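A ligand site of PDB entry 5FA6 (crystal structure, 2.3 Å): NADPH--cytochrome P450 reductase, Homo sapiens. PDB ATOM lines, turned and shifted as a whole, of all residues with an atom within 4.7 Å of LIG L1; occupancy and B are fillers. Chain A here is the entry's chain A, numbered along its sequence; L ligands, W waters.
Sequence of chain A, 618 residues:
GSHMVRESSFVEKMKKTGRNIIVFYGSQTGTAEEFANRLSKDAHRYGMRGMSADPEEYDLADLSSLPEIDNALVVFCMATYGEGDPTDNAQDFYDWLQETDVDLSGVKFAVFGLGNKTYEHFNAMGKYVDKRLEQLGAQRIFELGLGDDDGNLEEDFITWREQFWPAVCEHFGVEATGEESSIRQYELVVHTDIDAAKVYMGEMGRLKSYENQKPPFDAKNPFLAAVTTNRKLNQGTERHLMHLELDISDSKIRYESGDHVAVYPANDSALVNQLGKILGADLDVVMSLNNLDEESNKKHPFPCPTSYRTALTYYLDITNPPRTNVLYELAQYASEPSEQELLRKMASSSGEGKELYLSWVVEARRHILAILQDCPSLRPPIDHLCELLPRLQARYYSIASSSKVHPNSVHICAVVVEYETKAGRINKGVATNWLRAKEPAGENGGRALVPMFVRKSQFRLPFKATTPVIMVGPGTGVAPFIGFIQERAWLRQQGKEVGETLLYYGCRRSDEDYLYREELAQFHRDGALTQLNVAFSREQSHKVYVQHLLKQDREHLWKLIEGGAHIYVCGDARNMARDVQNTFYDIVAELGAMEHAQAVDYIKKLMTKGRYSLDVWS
Water W4 lies within hydrogen-bond range of an oxygen (O7) of LIG L1 (2.4 Å) and the backbone carbonyl oxygen of Val 415 (2.5 Å).
Water W3 bridges the side-chain hydroxyl (OH) of Tyr 419 (2.5 Å) and an oxygen (O4) of LIG L1 (2.7 Å).
Water W5 lies within hydrogen-bond range of the side-chain hydroxyl (OG1) of Thr 319 (2.7 Å), an oxygen (O1) of LIG L1 (2.8 Å) and the side-chain amide oxygen (OD1) of Asn 320 (2.8 Å).
Water W2 bridges an oxygen (O9) of LIG L1 (2.8 Å) and the backbone NH of Tyr 396 (2.8 Å).
Water W1 lies within hydrogen-bond range of N of Cys 413, O of Ser 398 and O8 of LIG L1.
Water W6 lies within hydrogen-bond range of an oxygen (O1) of LIG L1 (3.0 Å) and the backbone carbonyl oxygen (O) of Lys 428 (3.1 Å).
The backbone NH (N) of Tyr 396 sits at hydrogen-bond distance from an oxygen (O9) of LIG L1 (3.3 Å).
O of Tyr 396 is in hydrogen-bond range of O9 of LIG L1, 2.6 Å away.
The backbone NH of Thr 432 lies within hydrogen-bond range of an oxygen (O13) of LIG L1.
An oxygen (O13) of LIG L1 lies within hydrogen-bond range of the side-chain hydroxyl (OG1) of Thr 432 (2.8 Å).
The guanidinium group (NE) of Arg 395 is in salt-bridge range of an oxygen (O14) of LIG L1, at 2.8 Å.
O of Cys 413 is in hydrogen-bond range of N7 of LIG L1 (2.9 Å).
The backbone NH (N) of Ala 431 is in hydrogen-bond range of an oxygen (O14) of LIG L1 (2.9 Å).
The backbone NH (N) of Val 430 lies within hydrogen-bond range of an oxygen (O1) of LIG L1, at 2.9 Å.
A nitrogen (N5) of LIG L1 is in hydrogen-bond range of the guanidinium group (NE) of Arg 365, at 2.9 Å.
The backbone NH (N) of Ser 398 is in hydrogen-bond range of an oxygen (O8) of LIG L1 (3.0 Å).
A nitrogen (N8) of LIG L1 sits at hydrogen-bond distance from the side-chain hydroxyl of Ser 398, at 3.4 Å.
The side-chain hydroxyl (OH) of Tyr 397 lies within hydrogen-bond range of an oxygen (O11) of LIG L1 (3.0 Å).
The backbone NH of Val 415 lies within hydrogen-bond range of an oxygen (O7) of LIG L1 (3.2 Å).
N of Val 417 lies within hydrogen-bond range of OG1 of Thr 432 (3.1 Å).
The side-chain carboxylate (OD2) of Asp 615 lies within hydrogen-bond range of the side-chain hydroxyl (OG) of Ser 398, 2.8 Å away.
N of Gly 429 sits at hydrogen-bond distance from O of Val 417.
NE2 of His 260 is in hydrogen-bond range of OD1 of Asp 615 (3.0 Å).
The indole nitrogen of Trp 617 lies close to a nitrogen (N9) of LIG L1, 3.4 Å away.
Merely in contact with LIG L1: Ala 414, Tyr 419, Gly 429, Val 417, His 260 and Thr 476.
Hydrophobic or aromatic side chains that line LIG L1: Tyr 396, Tyr 397, Ala 414, Val 415, Val 417, Tyr 419, Val 430, Ala 431 and Trp 617.
Along chain A the residues within 4 Å of LIG L1 span positions 260 to 617.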
ATOM      1  N   HIS A 260     -14.908  24.544 -21.880  1.00  0.00           N
ATOM      2  CA  HIS A 260     -13.486  24.287 -21.972  1.00  0.00           C
ATOM      3  C   HIS A 260     -13.225  22.992 -22.706  1.00  0.00           C
ATOM      4  O   HIS A 260     -14.104  22.135 -22.797  1.00  0.00           O
ATOM      5  CB  HIS A 260     -12.877  24.214 -20.564  1.00  0.00           C
ATOM      6  CG  HIS A 260     -13.118  25.448 -19.761  1.00  0.00           C
ATOM      7  ND1 HIS A 260     -13.807  25.437 -18.560  1.00  0.00           N
ATOM      8  CD2 HIS A 260     -12.753  26.736 -19.964  1.00  0.00           C
ATOM      9  CE1 HIS A 260     -13.857  26.662 -18.064  1.00  0.00           C
ATOM     10  NE2 HIS A 260     -13.223  27.465 -18.898  1.00  0.00           N
ATOM     11  N   THR A 319       7.504  17.113 -14.664  1.00  0.00           N
ATOM     12  CA  THR A 319       7.914  18.493 -14.859  1.00  0.00           C
ATOM     13  C   THR A 319       7.685  19.457 -13.678  1.00  0.00           C
ATOM     14  O   THR A 319       8.493  20.361 -13.464  1.00  0.00           O
ATOM     15  CB  THR A 319       7.249  19.038 -16.129  1.00  0.00           C
ATOM     16  OG1 THR A 319       5.853  18.699 -16.116  1.00  0.00           O
ATOM     17  CG2 THR A 319       7.918  18.445 -17.388  1.00  0.00           C
ATOM     18  N   ASN A 320       6.604  19.292 -12.927  1.00  0.00           N
ATOM     19  CA  ASN A 320       6.348  20.194 -11.801  1.00  0.00           C
ATOM     20  C   ASN A 320       7.296  19.922 -10.642  1.00  0.00           C
ATOM     21  O   ASN A 320       7.716  18.788 -10.432  1.00  0.00           O
ATOM     22  CB  ASN A 320       4.914  20.076 -11.300  1.00  0.00           C
ATOM     23  CG  ASN A 320       3.915  20.662 -12.272  1.00  0.00           C
ATOM     24  OD1 ASN A 320       4.137  21.754 -12.818  1.00  0.00           O
ATOM     25  ND2 ASN A 320       2.803  19.949 -12.495  1.00  0.00           N
ATOM     26  N   ARG A 365      12.338  26.113  -9.977  1.00  0.00           N
ATOM     27  CA  ARG A 365      11.543  25.272 -10.865  1.00  0.00           C
ATOM     28  C   ARG A 365      12.276  23.990 -11.291  1.00  0.00           C
ATOM     29  O   ARG A 365      12.308  23.642 -12.464  1.00  0.00           O
ATOM     30  CB  ARG A 365      11.127  26.088 -12.085  1.00  0.00           C
ATOM     31  CG  ARG A 365      10.134  27.204 -11.767  1.00  0.00           C
ATOM     32  CD  ARG A 365       8.746  26.636 -11.582  1.00  0.00           C
ATOM     33  NE  ARG A 365       7.706  27.664 -11.672  1.00  0.00           N
ATOM     34  CZ  ARG A 365       7.491  28.607 -10.749  1.00  0.00           C
ATOM     35  NH1 ARG A 365       6.520  29.486 -10.931  1.00  0.00           N
ATOM     36  NH2 ARG A 365       8.236  28.657  -9.648  1.00  0.00           N
ATOM     37  N   ARG A 395      -4.862  19.260 -19.561  1.00  0.00           N
ATOM     38  CA  ARG A 395      -4.800  20.706 -19.479  1.00  0.00           C
ATOM     39  C   ARG A 395      -6.100  21.254 -20.063  1.00  0.00           C
ATOM     40  O   ARG A 395      -6.660  20.672 -21.005  1.00  0.00           O
ATOM     41  CB  ARG A 395      -3.597  21.253 -20.244  1.00  0.00           C
ATOM     42  CG  ARG A 395      -2.374  21.463 -19.377  1.00  0.00           C
ATOM     43  CD  ARG A 395      -1.797  20.180 -18.798  1.00  0.00           C
ATOM     44  NE  ARG A 395      -0.421  20.416 -18.327  1.00  0.00           N
ATOM     45  CZ  ARG A 395       0.293  19.554 -17.598  1.00  0.00           C
ATOM     46  NH1 ARG A 395       1.521  19.853 -17.228  1.00  0.00           N
ATOM     47  NH2 ARG A 395      -0.254  18.398 -17.238  1.00  0.00           N
ATOM     48  N   TYR A 396      -6.576  22.365 -19.510  1.00  0.00           N
ATOM     49  CA  TYR A 396      -7.813  22.970 -19.966  1.00  0.00           C
ATOM     50  C   TYR A 396      -7.595  24.216 -20.840  1.00  0.00           C
ATOM     51  O   TYR A 396      -6.701  25.010 -20.578  1.00  0.00           O
ATOM     52  CB  TYR A 396      -8.674  23.325 -18.744  1.00  0.00           C
ATOM     53  CG  TYR A 396      -9.211  22.104 -17.987  1.00  0.00           C
ATOM     54  CD1 TYR A 396     -10.263  21.347 -18.496  1.00  0.00           C
ATOM     55  CD2 TYR A 396      -8.651  21.717 -16.766  1.00  0.00           C
ATOM     56  CE1 TYR A 396     -10.754  20.223 -17.800  1.00  0.00           C
ATOM     57  CE2 TYR A 396      -9.132  20.606 -16.065  1.00  0.00           C
ATOM     58  CZ  TYR A 396     -10.181  19.858 -16.589  1.00  0.00           C
ATOM     59  OH  TYR A 396     -10.645  18.737 -15.927  1.00  0.00           O
ATOM     60  N   TYR A 397      -8.407  24.373 -21.872  1.00  0.00           N
ATOM     61  CA  TYR A 397      -8.303  25.533 -22.756  1.00  0.00           C
ATOM     62  C   TYR A 397      -9.694  26.030 -23.034  1.00  0.00           C
ATOM     63  O   TYR A 397     -10.634  25.242 -23.133  1.00  0.00           O
ATOM     64  CB  TYR A 397      -7.611  25.165 -24.078  1.00  0.00           C
ATOM     65  CG  TYR A 397      -6.181  24.752 -23.878  1.00  0.00           C
ATOM     66  CD1 TYR A 397      -5.169  25.719 -23.779  1.00  0.00           C
ATOM     67  CD2 TYR A 397      -5.863  23.426 -23.620  1.00  0.00           C
ATOM     68  CE1 TYR A 397      -3.873  25.364 -23.418  1.00  0.00           C
ATOM     69  CE2 TYR A 397      -4.572  23.051 -23.253  1.00  0.00           C
ATOM     70  CZ  TYR A 397      -3.580  24.024 -23.145  1.00  0.00           C
ATOM     71  OH  TYR A 397      -2.339  23.665 -22.714  1.00  0.00           O
ATOM     72  N   SER A 398      -9.836  27.353 -23.160  1.00  0.00           N
ATOM     73  CA  SER A 398     -11.134  27.952 -23.420  1.00  0.00           C
ATOM     74  C   SER A 398     -11.432  27.896 -24.922  1.00  0.00           C
ATOM     75  O   SER A 398     -10.794  28.569 -25.724  1.00  0.00           O
ATOM     76  CB  SER A 398     -11.117  29.396 -22.918  1.00  0.00           C
ATOM     77  OG  SER A 398     -10.687  29.446 -21.563  1.00  0.00           O
ATOM     78  N   CYS A 413      -6.759  28.485 -28.580  1.00  0.00           N
ATOM     79  CA  CYS A 413      -5.842  29.596 -28.699  1.00  0.00           C
ATOM     80  C   CYS A 413      -4.877  29.484 -27.522  1.00  0.00           C
ATOM     81  O   CYS A 413      -5.271  29.733 -26.390  1.00  0.00           O
ATOM     82  CB  CYS A 413      -6.572  30.941 -28.597  1.00  0.00           C
ATOM     83  SG  CYS A 413      -5.409  32.357 -28.426  1.00  0.00           S
ATOM     84  N   ALA A 414      -3.616  29.157 -27.784  1.00  0.00           N
ATOM     85  CA  ALA A 414      -2.686  29.001 -26.672  1.00  0.00           C
ATOM     86  C   ALA A 414      -1.300  29.599 -26.851  1.00  0.00           C
ATOM     87  O   ALA A 414      -0.784  29.707 -27.959  1.00  0.00           O
ATOM     88  CB  ALA A 414      -2.547  27.535 -26.318  1.00  0.00           C
ATOM     89  N   VAL A 415      -0.718  29.969 -25.702  1.00  0.00           N
ATOM     90  CA  VAL A 415       0.619  30.518 -25.649  1.00  0.00           C
ATOM     91  C   VAL A 415       1.519  29.398 -25.135  1.00  0.00           C
ATOM     92  O   VAL A 415       1.216  28.763 -24.113  1.00  0.00           O
ATOM     93  CB  VAL A 415       0.677  31.773 -24.729  1.00  0.00           C
ATOM     94  CG1 VAL A 415       0.217  31.440 -23.303  1.00  0.00           C
ATOM     95  CG2 VAL A 415       2.101  32.347 -24.698  1.00  0.00           C
ATOM     96  N   VAL A 417       4.494  27.630 -23.299  1.00  0.00           N
ATOM     97  CA  VAL A 417       5.330  27.918 -22.160  1.00  0.00           C
ATOM     98  C   VAL A 417       6.758  27.398 -22.328  1.00  0.00           C
ATOM     99  O   VAL A 417       6.995  26.216 -22.561  1.00  0.00           O
ATOM    100  CB  VAL A 417       4.718  27.314 -20.884  1.00  0.00           C
ATOM    101  CG1 VAL A 417       5.605  27.597 -19.689  1.00  0.00           C
ATOM    102  CG2 VAL A 417       3.333  27.887 -20.678  1.00  0.00           C
ATOM    103  N   TYR A 419      10.748  28.793 -20.713  1.00  0.00           N
ATOM    104  CA  TYR A 419      11.516  29.798 -19.988  1.00  0.00           C
ATOM    105  C   TYR A 419      12.781  29.180 -19.408  1.00  0.00           C
ATOM    106  O   TYR A 419      12.840  27.960 -19.209  1.00  0.00           O
ATOM    107  CB  TYR A 419      10.691  30.360 -18.831  1.00  0.00           C
ATOM    108  CG  TYR A 419      10.239  29.301 -17.842  1.00  0.00           C
ATOM    109  CD1 TYR A 419       9.177  28.440 -18.128  1.00  0.00           C
ATOM    110  CD2 TYR A 419      10.905  29.130 -16.631  1.00  0.00           C
ATOM    111  CE1 TYR A 419       8.795  27.428 -17.234  1.00  0.00           C
ATOM    112  CE2 TYR A 419      10.536  28.121 -15.733  1.00  0.00           C
ATOM    113  CZ  TYR A 419       9.475  27.279 -16.033  1.00  0.00           C
ATOM    114  OH  TYR A 419       9.111  26.292 -15.142  1.00  0.00           O
ATOM    115  N   LYS A 428      10.186  23.484 -20.321  1.00  0.00           N
ATOM    116  CA  LYS A 428       9.167  23.516 -21.359  1.00  0.00           C
ATOM    117  C   LYS A 428       7.826  23.019 -20.841  1.00  0.00           C
ATOM    118  O   LYS A 428       7.761  21.977 -20.207  1.00  0.00           O
ATOM    119  CB  LYS A 428       9.578  22.661 -22.542  1.00  0.00           C
ATOM    120  CG  LYS A 428      10.739  23.196 -23.353  1.00  0.00           C
ATOM    121  CD  LYS A 428      10.793  22.421 -24.646  1.00  0.00           C
ATOM    122  CE  LYS A 428      11.924  22.869 -25.549  1.00  0.00           C
ATOM    123  NZ  LYS A 428      11.747  22.198 -26.869  1.00  0.00           N
ATOM    124  N   GLY A 429       6.768  23.778 -21.129  1.00  0.00           N
ATOM    125  CA  GLY A 429       5.430  23.386 -20.709  1.00  0.00           C
ATOM    126  C   GLY A 429       5.032  22.093 -21.392  1.00  0.00           C
ATOM    127  O   GLY A 429       5.265  21.919 -22.577  1.00  0.00           O
ATOM    128  N   VAL A 430       4.387  21.196 -20.657  1.00  0.00           N
ATOM    129  CA  VAL A 430       4.039  19.921 -21.254  1.00  0.00           C
ATOM    130  C   VAL A 430       3.034  19.916 -22.391  1.00  0.00           C
ATOM    131  O   VAL A 430       3.324  19.463 -23.505  1.00  0.00           O
ATOM    132  CB  VAL A 430       3.572  18.907 -20.189  1.00  0.00           C
ATOM    133  CG1 VAL A 430       3.273  17.576 -20.842  1.00  0.00           C
ATOM    134  CG2 VAL A 430       4.662  18.729 -19.123  1.00  0.00           C
ATOM    135  N   ALA A 431       1.835  20.428 -22.147  1.00  0.00           N
ATOM    136  CA  ALA A 431       0.806  20.376 -23.186  1.00  0.00           C
ATOM    137  C   ALA A 431       0.990  21.354 -24.340  1.00  0.00           C
ATOM    138  O   ALA A 431       0.654  21.034 -25.498  1.00  0.00           O
ATOM    139  CB  ALA A 431      -0.590  20.545 -22.556  1.00  0.00           C
ATOM    140  N   THR A 432       1.497  22.552 -24.045  1.00  0.00           N
ATOM    141  CA  THR A 432       1.663  23.523 -25.123  1.00  0.00           C
ATOM    142  C   THR A 432       2.757  23.096 -26.092  1.00  0.00           C
ATOM    143  O   THR A 432       2.551  23.147 -27.299  1.00  0.00           O
ATOM    144  CB  THR A 432       1.914  24.958 -24.579  1.00  0.00           C
ATOM    145  OG1 THR A 432       3.070  24.967 -23.733  1.00  0.00           O
ATOM    146  CG2 THR A 432       0.679  25.462 -23.783  1.00  0.00           C
ATOM    147  N   THR A 476      -4.129  35.599 -24.265  1.00  0.00           N
ATOM    148  CA  THR A 476      -4.887  34.405 -24.614  1.00  0.00           C
ATOM    149  C   THR A 476      -6.285  34.457 -24.028  1.00  0.00           C
ATOM    150  O   THR A 476      -7.122  33.639 -24.345  1.00  0.00           O
ATOM    151  CB  THR A 476      -4.166  33.120 -24.156  1.00  0.00           C
ATOM    152  OG1 THR A 476      -3.865  33.188 -22.758  1.00  0.00           O
ATOM    153  CG2 THR A 476      -2.900  32.930 -24.946  1.00  0.00           C
ATOM    154  N   ALA A 479      -9.547  34.130 -26.147  1.00  0.00           N
ATOM    155  CA  ALA A 479     -10.061  32.877 -26.685  1.00  0.00           C
ATOM    156  C   ALA A 479     -11.566  32.646 -26.698  1.00  0.00           C
ATOM    157  O   ALA A 479     -12.156  32.487 -27.771  1.00  0.00           O
ATOM    158  CB  ALA A 479      -9.352  31.692 -26.006  1.00  0.00           C
ATOM    159  N   ASP A 615     -13.738  33.692 -16.484  1.00  0.00           N
ATOM    160  CA  ASP A 615     -13.080  32.517 -17.029  1.00  0.00           C
ATOM    161  C   ASP A 615     -11.606  32.870 -16.946  1.00  0.00           C
ATOM    162  O   ASP A 615     -10.978  33.258 -17.935  1.00  0.00           O
ATOM    163  CB  ASP A 615     -13.475  32.269 -18.496  1.00  0.00           C
ATOM    164  CG  ASP A 615     -12.723  31.087 -19.105  1.00  0.00           C
ATOM    165  OD1 ASP A 615     -12.202  30.251 -18.328  1.00  0.00           O
ATOM    166  OD2 ASP A 615     -12.668  31.004 -20.349  1.00  0.00           O
ATOM    167  N   TRP A 617      -7.508  32.054 -15.203  1.00  0.00           N
ATOM    168  CA  TRP A 617      -6.533  31.044 -14.776  1.00  0.00           C
ATOM    169  C   TRP A 617      -5.152  31.676 -14.580  1.00  0.00           C
ATOM    170  O   TRP A 617      -4.926  32.854 -14.878  1.00  0.00           O
ATOM    171  CB  TRP A 617      -6.438  29.941 -15.838  1.00  0.00           C
ATOM    172  CG  TRP A 617      -5.869  30.406 -17.181  1.00  0.00           C
ATOM    173  CD1 TRP A 617      -4.540  30.463 -17.545  1.00  0.00           C
ATOM    174  CD2 TRP A 617      -6.610  30.888 -18.305  1.00  0.00           C
ATOM    175  NE1 TRP A 617      -4.412  30.957 -18.817  1.00  0.00           N
ATOM    176  CE2 TRP A 617      -5.659  31.217 -19.317  1.00  0.00           C
ATOM    177  CE3 TRP A 617      -7.976  31.063 -18.568  1.00  0.00           C
ATOM    178  CZ2 TRP A 617      -6.050  31.718 -20.568  1.00  0.00           C
ATOM    179  CZ3 TRP A 617      -8.363  31.565 -19.810  1.00  0.00           C
ATOM    180  CH2 TRP A 617      -7.392  31.890 -20.807  1.00  0.00           C
ATOM    181  N   SER A 618      -4.212  30.870 -14.087  1.00  0.00           N
ATOM    182  CA  SER A 618      -2.842  31.337 -13.878  1.00  0.00           C
ATOM    183  C   SER A 618      -1.925  30.131 -13.778  1.00  0.00           C
ATOM    184  O   SER A 618      -2.434  28.990 -13.893  1.00  0.00           O
ATOM    185  CB  SER A 618      -2.742  32.182 -12.612  1.00  0.00           C
ATOM    186  OG  SER A 618      -3.326  31.507 -11.512  1.00  0.00           O
ATOM    187  OXT SER A 618      -0.706  30.339 -13.598  1.00  0.00           O
HETATM  188  P1  LIG L   1       2.995  23.159 -17.592  1.00  0.00           P
HETATM  189  O1  LIG L   1       3.989  22.125 -17.926  1.00  0.00           O
HETATM  190  O2  LIG L   1       1.698  22.751 -16.999  1.00  0.00           O
HETATM  191  O3  LIG L   1       3.674  24.259 -16.645  1.00  0.00           O
HETATM  192  C1  LIG L   1       2.933  25.413 -16.257  1.00  0.00           C
HETATM  193  C2  LIG L   1       3.655  26.158 -15.130  1.00  0.00           C
HETATM  194  O4  LIG L   1       4.952  26.614 -15.543  1.00  0.00           O
HETATM  195  C3  LIG L   1       2.946  27.466 -14.809  1.00  0.00           C
HETATM  196  O5  LIG L   1       1.775  27.204 -14.022  1.00  0.00           O
HETATM  197  C4  LIG L   1       4.013  28.076 -13.923  1.00  0.00           C
HETATM  198  O6  LIG L   1       3.946  27.487 -12.605  1.00  0.00           O
HETATM  199  C5  LIG L   1       5.303  27.674 -14.618  1.00  0.00           C
HETATM  200  N1  LIG L   1       5.835  28.787 -15.420  1.00  0.00           N
HETATM  201  C6  LIG L   1       5.241  29.340 -16.656  1.00  0.00           C
HETATM  202  N2  LIG L   1       6.142  30.476 -16.917  1.00  0.00           N
HETATM  203  C7  LIG L   1       7.108  30.473 -16.005  1.00  0.00           C
HETATM  204  C8  LIG L   1       8.127  31.312 -15.863  1.00  0.00           C
HETATM  205  N3  LIG L   1       8.479  31.982 -16.957  1.00  0.00           N
HETATM  206  N4  LIG L   1       8.865  31.373 -14.749  1.00  0.00           N
HETATM  207  C9  LIG L   1       8.581  30.488 -13.701  1.00  0.00           C
HETATM  208  N5  LIG L   1       7.526  29.585 -13.893  1.00  0.00           N
HETATM  209  C10 LIG L   1       6.819  29.600 -15.035  1.00  0.00           C
HETATM  210  N6  LIG L   1      -3.960  28.717 -21.553  1.00  0.00           N
HETATM  211  C11 LIG L   1      -3.964  29.168 -22.880  1.00  0.00           C
HETATM  212  O7  LIG L   1      -2.913  29.372 -23.469  1.00  0.00           O
HETATM  213  N7  LIG L   1      -5.186  29.304 -23.557  1.00  0.00           N
HETATM  214  C12 LIG L   1      -6.385  29.013 -22.907  1.00  0.00           C
HETATM  215  O8  LIG L   1      -7.450  29.136 -23.519  1.00  0.00           O
HETATM  216  C13 LIG L   1      -6.376  28.562 -21.593  1.00  0.00           C
HETATM  217  N8  LIG L   1      -7.522  28.491 -20.898  1.00  0.00           N
HETATM  218  C14 LIG L   1      -7.506  28.036 -19.642  1.00  0.00           C
HETATM  219  C15 LIG L   1      -8.707  27.840 -18.965  1.00  0.00           C
HETATM  220  C16 LIG L   1      -8.732  27.209 -17.736  1.00  0.00           C
HETATM  221  C17 LIG L   1      -9.948  26.933 -17.115  1.00  0.00           C
HETATM  222  C18 LIG L   1      -7.531  26.784 -17.152  1.00  0.00           C
HETATM  223  C19 LIG L   1      -7.553  26.058 -15.973  1.00  0.00           C
HETATM  224  C20 LIG L   1      -6.327  27.013 -17.814  1.00  0.00           C
HETATM  225  C21 LIG L   1      -6.309  27.630 -19.060  1.00  0.00           C
HETATM  226  N9  LIG L   1      -5.167  27.741 -19.750  1.00  0.00           N
HETATM  227  C22 LIG L   1      -5.174  28.411 -20.916  1.00  0.00           C
HETATM  228  C23 LIG L   1      -3.880  27.323 -19.173  1.00  0.00           C
HETATM  229  C24 LIG L   1      -3.533  25.904 -19.656  1.00  0.00           C
HETATM  230  O9  LIG L   1      -4.527  24.978 -19.237  1.00  0.00           O
HETATM  231  C25 LIG L   1      -2.156  25.456 -19.158  1.00  0.00           C
HETATM  232  O10 LIG L   1      -2.021  25.685 -17.749  1.00  0.00           O
HETATM  233  C26 LIG L   1      -1.075  26.235 -19.911  1.00  0.00           C
HETATM  234  O11 LIG L   1      -1.290  26.103 -21.314  1.00  0.00           O
HETATM  235  C27 LIG L   1       0.307  25.685 -19.531  1.00  0.00           C
HETATM  236  O12 LIG L   1       0.284  24.259 -19.712  1.00  0.00           O
HETATM  237  P2  LIG L   1       1.638  23.453 -20.038  1.00  0.00           P
HETATM  238  O13 LIG L   1       2.133  23.853 -21.370  1.00  0.00           O
HETATM  239  O14 LIG L   1       1.362  22.014 -19.792  1.00  0.00           O
HETATM  240  O15 LIG L   1       2.671  24.004 -18.937  1.00  0.00           O
HETATM  241  N1  LG2 L   2      -9.879  27.984  -5.641  1.00  0.00           N
HETATM  242  C1  LG2 L   2     -10.739  28.680  -4.838  1.00  0.00           C
HETATM  243  O1  LG2 L   2     -10.466  28.976  -3.681  1.00  0.00           O
HETATM  244  N2  LG2 L   2     -11.957  29.053  -5.404  1.00  0.00           N
HETATM  245  C2  LG2 L   2     -12.386  28.802  -6.710  1.00  0.00           C
HETATM  246  O2  LG2 L   2     -13.498  29.225  -6.967  1.00  0.00           O
HETATM  247  C3  LG2 L   2     -11.499  28.088  -7.556  1.00  0.00           C
HETATM  248  N3  LG2 L   2     -11.932  27.836  -8.871  1.00  0.00           N
HETATM  249  C4  LG2 L   2     -11.020  27.131  -9.662  1.00  0.00           C
HETATM  250  C5  LG2 L   2     -11.439  26.879 -11.017  1.00  0.00           C
HETATM  251  C6  LG2 L   2     -10.605  26.187 -11.943  1.00  0.00           C
HETATM  252  C7  LG2 L   2     -11.176  25.989 -13.362  1.00  0.00           C
HETATM  253  C8  LG2 L   2      -9.261  25.685 -11.509  1.00  0.00           C
HETATM  254  C9  LG2 L   2      -8.365  24.987 -12.306  1.00  0.00           C
HETATM  255  C10 LG2 L   2      -8.841  25.912 -10.206  1.00  0.00           C
HETATM  256  C11 LG2 L   2      -9.698  26.644  -9.244  1.00  0.00           C
HETATM  257  N4  LG2 L   2      -9.315  26.935  -7.836  1.00  0.00           N
HETATM  258  C12 LG2 L   2     -10.249  27.694  -6.955  1.00  0.00           C
HETATM  259  C13 LG2 L   2      -8.021  26.468  -7.353  1.00  0.00           C
HETATM  260  C14 LG2 L   2      -8.038  24.994  -6.838  1.00  0.00           C
HETATM  261  O3  LG2 L   2      -9.011  24.907  -5.717  1.00  0.00           O
HETATM  262  C15 LG2 L   2      -6.653  24.575  -6.383  1.00  0.00           C
HETATM  263  O4  LG2 L   2      -5.790  24.667  -7.545  1.00  0.00           O
HETATM  264  C16 LG2 L   2      -6.705  23.087  -5.828  1.00  0.00           C
HETATM  265  O5  LG2 L   2      -5.303  22.902  -5.424  1.00  0.00           O
HETATM  266  C17 LG2 L   2      -6.977  21.992  -6.860  1.00  0.00           C
HETATM  267  O6  LG2 L   2      -7.049  20.654  -6.201  1.00  0.00           O
HETATM  268  P1  LG2 L   2      -7.281  19.249  -6.904  1.00  0.00           P
HETATM  269  O7  LG2 L   2      -6.106  18.904  -7.725  1.00  0.00           O
HETATM  270  O8  LG2 L   2      -8.687  19.368  -7.573  1.00  0.00           O
HETATM  271  O9  LG2 L   2      -7.297  18.266  -5.636  1.00  0.00           O
HETATM  272  O   HOH W   1      -8.046  27.879 -26.143  1.00  0.00           O
HETATM  273  O   HOH W   2      -5.358  23.289 -17.126  1.00  0.00           O
HETATM  274  O   HOH W   3       7.117  24.957 -15.799  1.00  0.00           O
HETATM  275  O   HOH W   4      -0.837  28.375 -22.706  1.00  0.00           O
HETATM  276  O   HOH W   5       4.582  20.964 -15.497  1.00  0.00           O
HETATM  277  O   HOH W   6       6.914  22.411 -17.271  1.00  0.00           O
